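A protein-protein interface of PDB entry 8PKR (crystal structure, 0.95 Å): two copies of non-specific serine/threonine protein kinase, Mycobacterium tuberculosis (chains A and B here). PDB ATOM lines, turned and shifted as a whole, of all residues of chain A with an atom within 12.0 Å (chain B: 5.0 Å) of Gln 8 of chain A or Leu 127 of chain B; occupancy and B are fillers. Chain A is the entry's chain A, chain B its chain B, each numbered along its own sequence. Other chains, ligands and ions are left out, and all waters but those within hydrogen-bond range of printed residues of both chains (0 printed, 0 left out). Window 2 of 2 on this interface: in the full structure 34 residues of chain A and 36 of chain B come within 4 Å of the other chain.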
ATOM      1  N   GLN A   8     -32.792  11.962 -23.056  1.00  0.00           N
ATOM      2  CA  GLN A   8     -31.521  11.794 -23.789  1.00  0.00           C
ATOM      3  C   GLN A   8     -30.909  13.173 -24.021  1.00  0.00           C
ATOM      4  O   GLN A   8     -31.643  14.065 -24.481  1.00  0.00           O
ATOM      5  CB  GLN A   8     -31.743  11.071 -25.116  1.00  0.00           C
ATOM      6  CG  GLN A   8     -30.477  11.082 -25.952  1.00  0.00           C
ATOM      7  CD  GLN A   8     -30.559  10.155 -27.128  1.00  0.00           C
ATOM      8  OE1 GLN A   8     -30.718   8.959 -26.961  1.00  0.00           O
ATOM      9  NE2 GLN A   8     -30.442  10.702 -28.322  1.00  0.00           N
ATOM     10  N   THR A   9     -29.611  13.324 -23.762  1.00  0.00           N
ATOM     11  CA  THR A   9     -28.918  14.595 -24.037  1.00  0.00           C
ATOM     12  C   THR A   9     -27.498  14.371 -24.569  1.00  0.00           C
ATOM     13  O   THR A   9     -26.848  13.484 -24.161  1.00  0.00           O
ATOM     14  CB  THR A   9     -28.858  15.483 -22.792  1.00  0.00           C
ATOM     15  OG1 THR A   9     -28.191  14.782 -21.745  1.00  0.00           O
ATOM     16  CG2 THR A   9     -30.223  15.929 -22.313  1.00  0.00           C
ATOM     17  N   VAL A  10     -27.051  15.171 -25.498  1.00  0.00           N
ATOM     18  CA  VAL A  10     -25.661  15.206 -25.942  1.00  0.00           C
ATOM     19  C   VAL A  10     -24.887  16.079 -24.972  1.00  0.00           C
ATOM     20  O   VAL A  10     -25.256  17.235 -24.731  1.00  0.00           O
ATOM     21  CB  VAL A  10     -25.567  15.755 -27.377  1.00  0.00           C
ATOM     22  CG1 VAL A  10     -24.104  15.878 -27.813  1.00  0.00           C
ATOM     23  CG2 VAL A  10     -26.356  14.878 -28.338  1.00  0.00           C
ATOM     24  N   LEU A  11     -23.819  15.548 -24.406  1.00  0.00           N
ATOM     25  CA  LEU A  11     -23.026  16.328 -23.473  1.00  0.00           C
ATOM     26  C   LEU A  11     -22.139  17.297 -24.255  1.00  0.00           C
ATOM     27  O   LEU A  11     -21.640  16.952 -25.332  1.00  0.00           O
ATOM     28  CB  LEU A  11     -22.178  15.416 -22.592  1.00  0.00           C
ATOM     29  CG  LEU A  11     -22.997  14.504 -21.669  1.00  0.00           C
ATOM     30  CD1 LEU A  11     -22.048  13.772 -20.727  1.00  0.00           C
ATOM     31  CD2 LEU A  11     -24.085  15.251 -20.891  1.00  0.00           C
ATOM     32  N   PRO A  12     -21.937  18.516 -23.743  1.00  0.00           N
ATOM     33  CA  PRO A  12     -21.277  19.572 -24.522  1.00  0.00           C
ATOM     34  C   PRO A  12     -19.747  19.506 -24.547  1.00  0.00           C
ATOM     35  O   PRO A  12     -19.061  20.507 -24.385  1.00  0.00           O
ATOM     36  CB  PRO A  12     -21.805  20.851 -23.860  1.00  0.00           C
ATOM     37  CG  PRO A  12     -22.002  20.453 -22.436  1.00  0.00           C
ATOM     38  CD  PRO A  12     -22.547  19.048 -22.507  1.00  0.00           C
ATOM     39  N   PHE A  13     -19.205  18.321 -24.810  1.00  0.00           N
ATOM     40  CA  PHE A  13     -17.811  18.250 -25.221  1.00  0.00           C
ATOM     41  C   PHE A  13     -17.627  18.992 -26.540  1.00  0.00           C
ATOM     42  O   PHE A  13     -18.561  19.155 -27.322  1.00  0.00           O
ATOM     43  CB  PHE A  13     -17.384  16.789 -25.408  1.00  0.00           C
ATOM     44  CG  PHE A  13     -17.250  16.019 -24.123  1.00  0.00           C
ATOM     45  CD1 PHE A  13     -16.072  16.063 -23.396  1.00  0.00           C
ATOM     46  CD2 PHE A  13     -18.287  15.234 -23.651  1.00  0.00           C
ATOM     47  CE1 PHE A  13     -15.933  15.344 -22.224  1.00  0.00           C
ATOM     48  CE2 PHE A  13     -18.155  14.523 -22.470  1.00  0.00           C
ATOM     49  CZ  PHE A  13     -16.974  14.570 -21.757  1.00  0.00           C
ATOM     50  N   LEU A  22     -15.131   5.687 -22.297  1.00  0.00           N
ATOM     51  CA  LEU A  22     -15.459   6.776 -21.397  1.00  0.00           C
ATOM     52  C   LEU A  22     -15.695   6.223 -20.000  1.00  0.00           C
ATOM     53  O   LEU A  22     -15.919   5.017 -19.801  1.00  0.00           O
ATOM     54  CB  LEU A  22     -16.637   7.639 -21.891  1.00  0.00           C
ATOM     55  CG  LEU A  22     -18.054   7.088 -21.713  1.00  0.00           C
ATOM     56  CD1 LEU A  22     -19.049   8.157 -22.180  1.00  0.00           C
ATOM     57  CD2 LEU A  22     -18.298   5.774 -22.440  1.00  0.00           C
ATOM     58  N   VAL A  24     -17.225   7.555 -15.805  1.00  0.00           N
ATOM     59  CA  VAL A  24     -17.980   8.532 -15.022  1.00  0.00           C
ATOM     60  C   VAL A  24     -17.630   8.320 -13.556  1.00  0.00           C
ATOM     61  O   VAL A  24     -17.616   7.184 -13.075  1.00  0.00           O
ATOM     62  CB  VAL A  24     -19.499   8.439 -15.303  1.00  0.00           C
ATOM     63  CG1 VAL A  24     -20.066   7.040 -14.990  1.00  0.00           C
ATOM     64  CG2 VAL A  24     -20.242   9.551 -14.574  1.00  0.00           C
ATOM     65  N   GLY A  28     -20.356  12.428 -11.042  1.00  0.00           N
ATOM     66  CA  GLY A  28     -20.974  12.637 -12.338  1.00  0.00           C
ATOM     67  C   GLY A  28     -20.105  13.300 -13.381  1.00  0.00           C
ATOM     68  O   GLY A  28     -20.613  13.615 -14.467  1.00  0.00           O
ATOM     69  N   VAL A  30     -17.626  13.201 -16.431  1.00  0.00           N
ATOM     70  CA  VAL A  30     -17.448  12.243 -17.515  1.00  0.00           C
ATOM     71  C   VAL A  30     -16.079  12.468 -18.138  1.00  0.00           C
ATOM     72  O   VAL A  30     -15.670  13.613 -18.385  1.00  0.00           O
ATOM     73  CB  VAL A  30     -18.580  12.364 -18.557  1.00  0.00           C
ATOM     74  CG1 VAL A  30     -18.351  11.446 -19.745  1.00  0.00           C
ATOM     75  CG2 VAL A  30     -19.920  12.032 -17.906  1.00  0.00           C
ATOM     76  N   LEU B  95     -32.446  -0.165 -24.817  1.00  0.00           N
ATOM     77  CA  LEU B  95     -32.619   1.122 -24.162  1.00  0.00           C
ATOM     78  C   LEU B  95     -33.147   2.156 -25.153  1.00  0.00           C
ATOM     79  O   LEU B  95     -32.795   2.132 -26.338  1.00  0.00           O
ATOM     80  CB  LEU B  95     -31.319   1.616 -23.559  1.00  0.00           C
ATOM     81  CG  LEU B  95     -30.775   0.751 -22.430  1.00  0.00           C
ATOM     82  CD1 LEU B  95     -29.547   1.425 -21.843  1.00  0.00           C
ATOM     83  CD2 LEU B  95     -31.815   0.477 -21.360  1.00  0.00           C
ATOM     84  N   PRO B  96     -33.995   3.080 -24.681  1.00  0.00           N
ATOM     85  CA  PRO B  96     -34.689   4.029 -25.560  1.00  0.00           C
ATOM     86  C   PRO B  96     -33.850   5.223 -26.020  1.00  0.00           C
ATOM     87  O   PRO B  96     -34.269   6.379 -25.919  1.00  0.00           O
ATOM     88  CB  PRO B  96     -35.874   4.478 -24.698  1.00  0.00           C
ATOM     89  CG  PRO B  96     -35.370   4.368 -23.301  1.00  0.00           C
ATOM     90  CD  PRO B  96     -34.514   3.141 -23.299  1.00  0.00           C
ATOM     91  N   PHE B  97     -32.649   4.946 -26.519  1.00  0.00           N
ATOM     92  CA  PHE B  97     -31.911   5.969 -27.237  1.00  0.00           C
ATOM     93  C   PHE B  97     -32.640   6.285 -28.535  1.00  0.00           C
ATOM     94  O   PHE B  97     -33.266   5.415 -29.152  1.00  0.00           O
ATOM     95  CB  PHE B  97     -30.503   5.491 -27.582  1.00  0.00           C
ATOM     96  CG  PHE B  97     -29.543   5.488 -26.419  1.00  0.00           C
ATOM     97  CD1 PHE B  97     -28.858   6.639 -26.058  1.00  0.00           C
ATOM     98  CD2 PHE B  97     -29.304   4.326 -25.703  1.00  0.00           C
ATOM     99  CE1 PHE B  97     -27.966   6.632 -24.992  1.00  0.00           C
ATOM    100  CE2 PHE B  97     -28.413   4.309 -24.647  1.00  0.00           C
ATOM    101  CZ  PHE B  97     -27.739   5.457 -24.290  1.00  0.00           C
ATOM    102  N   THR B  98     -32.547   7.540 -28.953  1.00  0.00           N
ATOM    103  CA  THR B  98     -33.151   8.007 -30.193  1.00  0.00           C
ATOM    104  C   THR B  98     -32.047   8.465 -31.133  1.00  0.00           C
ATOM    105  O   THR B  98     -31.141   9.195 -30.719  1.00  0.00           O
ATOM    106  CB  THR B  98     -34.123   9.159 -29.916  1.00  0.00           C
ATOM    107  OG1 THR B  98     -33.456  10.185 -29.174  1.00  0.00           O
ATOM    108  CG2 THR B  98     -35.321   8.673 -29.119  1.00  0.00           C
ATOM    109  N   ILE B 100     -29.417   7.210 -32.544  1.00  0.00           N
ATOM    110  CA  ILE B 100     -28.014   6.888 -32.299  1.00  0.00           C
ATOM    111  C   ILE B 100     -27.520   5.901 -33.350  1.00  0.00           C
ATOM    112  O   ILE B 100     -28.249   4.994 -33.771  1.00  0.00           O
ATOM    113  CB  ILE B 100     -27.790   6.357 -30.870  1.00  0.00           C
ATOM    114  CG1 ILE B 100     -28.520   5.030 -30.653  1.00  0.00           C
ATOM    115  CG2 ILE B 100     -28.244   7.401 -29.852  1.00  0.00           C
ATOM    116  CD1 ILE B 100     -27.923   4.209 -29.571  1.00  0.00           C
ATOM    117  N   GLY B 112     -27.557   4.807 -12.232  1.00  0.00           N
ATOM    118  CA  GLY B 112     -28.023   3.988 -13.333  1.00  0.00           C
ATOM    119  C   GLY B 112     -28.097   4.712 -14.658  1.00  0.00           C
ATOM    120  O   GLY B 112     -28.593   4.149 -15.639  1.00  0.00           O
ATOM    121  N   THR B 113     -27.631   5.954 -14.715  1.00  0.00           N
ATOM    122  CA  THR B 113     -27.623   6.689 -15.967  1.00  0.00           C
ATOM    123  C   THR B 113     -26.536   6.118 -16.868  1.00  0.00           C
ATOM    124  O   THR B 113     -25.428   5.810 -16.416  1.00  0.00           O
ATOM    125  CB  THR B 113     -27.389   8.168 -15.689  1.00  0.00           C
ATOM    126  OG1 THR B 113     -28.476   8.659 -14.892  1.00  0.00           O
ATOM    127  CG2 THR B 113     -27.286   8.980 -16.971  1.00  0.00           C
ATOM    128  N   VAL B 114     -26.879   5.956 -18.145  1.00  0.00           N
ATOM    129  CA  VAL B 114     -26.014   5.339 -19.138  1.00  0.00           C
ATOM    130  C   VAL B 114     -25.418   6.427 -20.014  1.00  0.00           C
ATOM    131  O   VAL B 114     -26.119   7.336 -20.464  1.00  0.00           O
ATOM    132  CB  VAL B 114     -26.818   4.328 -19.984  1.00  0.00           C
ATOM    133  CG1 VAL B 114     -25.973   3.776 -21.087  1.00  0.00           C
ATOM    134  CG2 VAL B 114     -27.342   3.214 -19.096  1.00  0.00           C
ATOM    135  N   VAL B 125     -23.263  10.801 -25.438  1.00  0.00           N
ATOM    136  CA  VAL B 125     -24.697  10.871 -25.229  1.00  0.00           C
ATOM    137  C   VAL B 125     -25.043  10.244 -23.894  1.00  0.00           C
ATOM    138  O   VAL B 125     -24.573   9.145 -23.570  1.00  0.00           O
ATOM    139  CB  VAL B 125     -25.445  10.216 -26.397  1.00  0.00           C
ATOM    140  CG1 VAL B 125     -26.949  10.448 -26.301  1.00  0.00           C
ATOM    141  CG2 VAL B 125     -24.903  10.766 -27.721  1.00  0.00           C
ATOM    142  N   LYS B 126     -25.893  10.931 -23.130  1.00  0.00           N
ATOM    143  CA  LYS B 126     -26.359  10.496 -21.805  1.00  0.00           C
ATOM    144  C   LYS B 126     -27.837  10.109 -21.899  1.00  0.00           C
ATOM    145  O   LYS B 126     -28.574  10.813 -22.523  1.00  0.00           O
ATOM    146  CB  LYS B 126     -26.161  11.675 -20.853  1.00  0.00           C
ATOM    147  CG  LYS B 126     -26.629  11.486 -19.427  1.00  0.00           C
ATOM    148  CD  LYS B 126     -26.450  12.783 -18.716  1.00  0.00           C
ATOM    149  CE  LYS B 126     -26.876  12.763 -17.273  1.00  0.00           C
ATOM    150  NZ  LYS B 126     -27.124  14.151 -16.816  1.00  0.00           N
ATOM    151  N   LEU B 127     -28.251   9.013 -21.281  1.00  0.00           N
ATOM    152  CA  LEU B 127     -29.677   8.599 -21.198  1.00  0.00           C
ATOM    153  C   LEU B 127     -30.076   8.413 -19.728  1.00  0.00           C
ATOM    154  O   LEU B 127     -29.504   7.531 -19.085  1.00  0.00           O
ATOM    155  CB  LEU B 127     -29.860   7.304 -21.983  1.00  0.00           C
ATOM    156  CG  LEU B 127     -31.312   6.852 -22.147  1.00  0.00           C
ATOM    157  CD1 LEU B 127     -32.129   7.887 -22.907  1.00  0.00           C
ATOM    158  CD2 LEU B 127     -31.388   5.514 -22.854  1.00  0.00           C
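The side-chain amide nitrogen of Gln 8 of chain A lies within hydrogen-bond range of the backbone carbonyl oxygen of Thr 98 of chain B, at 2.9 Å. The backbone carbonyl oxygen of Thr 9 of chain A lies within hydrogen-bond range of the backbone NH of Lys 126 of chain B (2.9 Å).
The backbone carbonyl oxygen of Val 114 of chain B is in hydrogen-bond range of the backbone NH of Leu 127 of chain B (2.8 Å).
Gln 8 of chain A touches Phe 97 of chain B. CG1 of Val 125 of chain B touches CG of Gln 8 of chain A, at 3.6 Å. Lys 126 of chain B touches Gln 8 of chain A (O to CA, 3.4 Å). Leu 127 of chain B touches Gln 8 of chain A. Thr 9 of chain A touches Val 125 of chain B.
Leu 127 of chain B touches just one residue of chain A: Gln 8 (3.9 Å). Leu 95 of chain B touches none of the printed residues of chain A. Of chain A, only Gln 8 comes within 4 Å of Phe 97 of chain B. No residue of chain A comes within 4 Å of Gly 112 of chain B. No residue of chain A comes within 4 Å of Thr 113 of chain B. Printed residues of chain B within 4 Å of Thr 9 of chain A: Val 125 (3.5 Å) and Lys 126 (2.9 Å). Val 30 of chain A touches none of the printed residues of chain B. The nearest residue of chain A that does not touch Leu 127 of chain B is Thr 9 of chain A (5.2 Å).
Hydrophobic or aromatic side chains of chain B that line the printed part of chain A: Phe 97, Val 125 and Leu 127. Among the printed residues, no Asp or Glu carboxylate lies within 4 Å of a Lys or Arg side-chain nitrogen of the other chain.
No position is printed for both chains. Of the 7 pairs that touch across the chains among the printed residues, none has its exchanged pair printed and touching as well.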
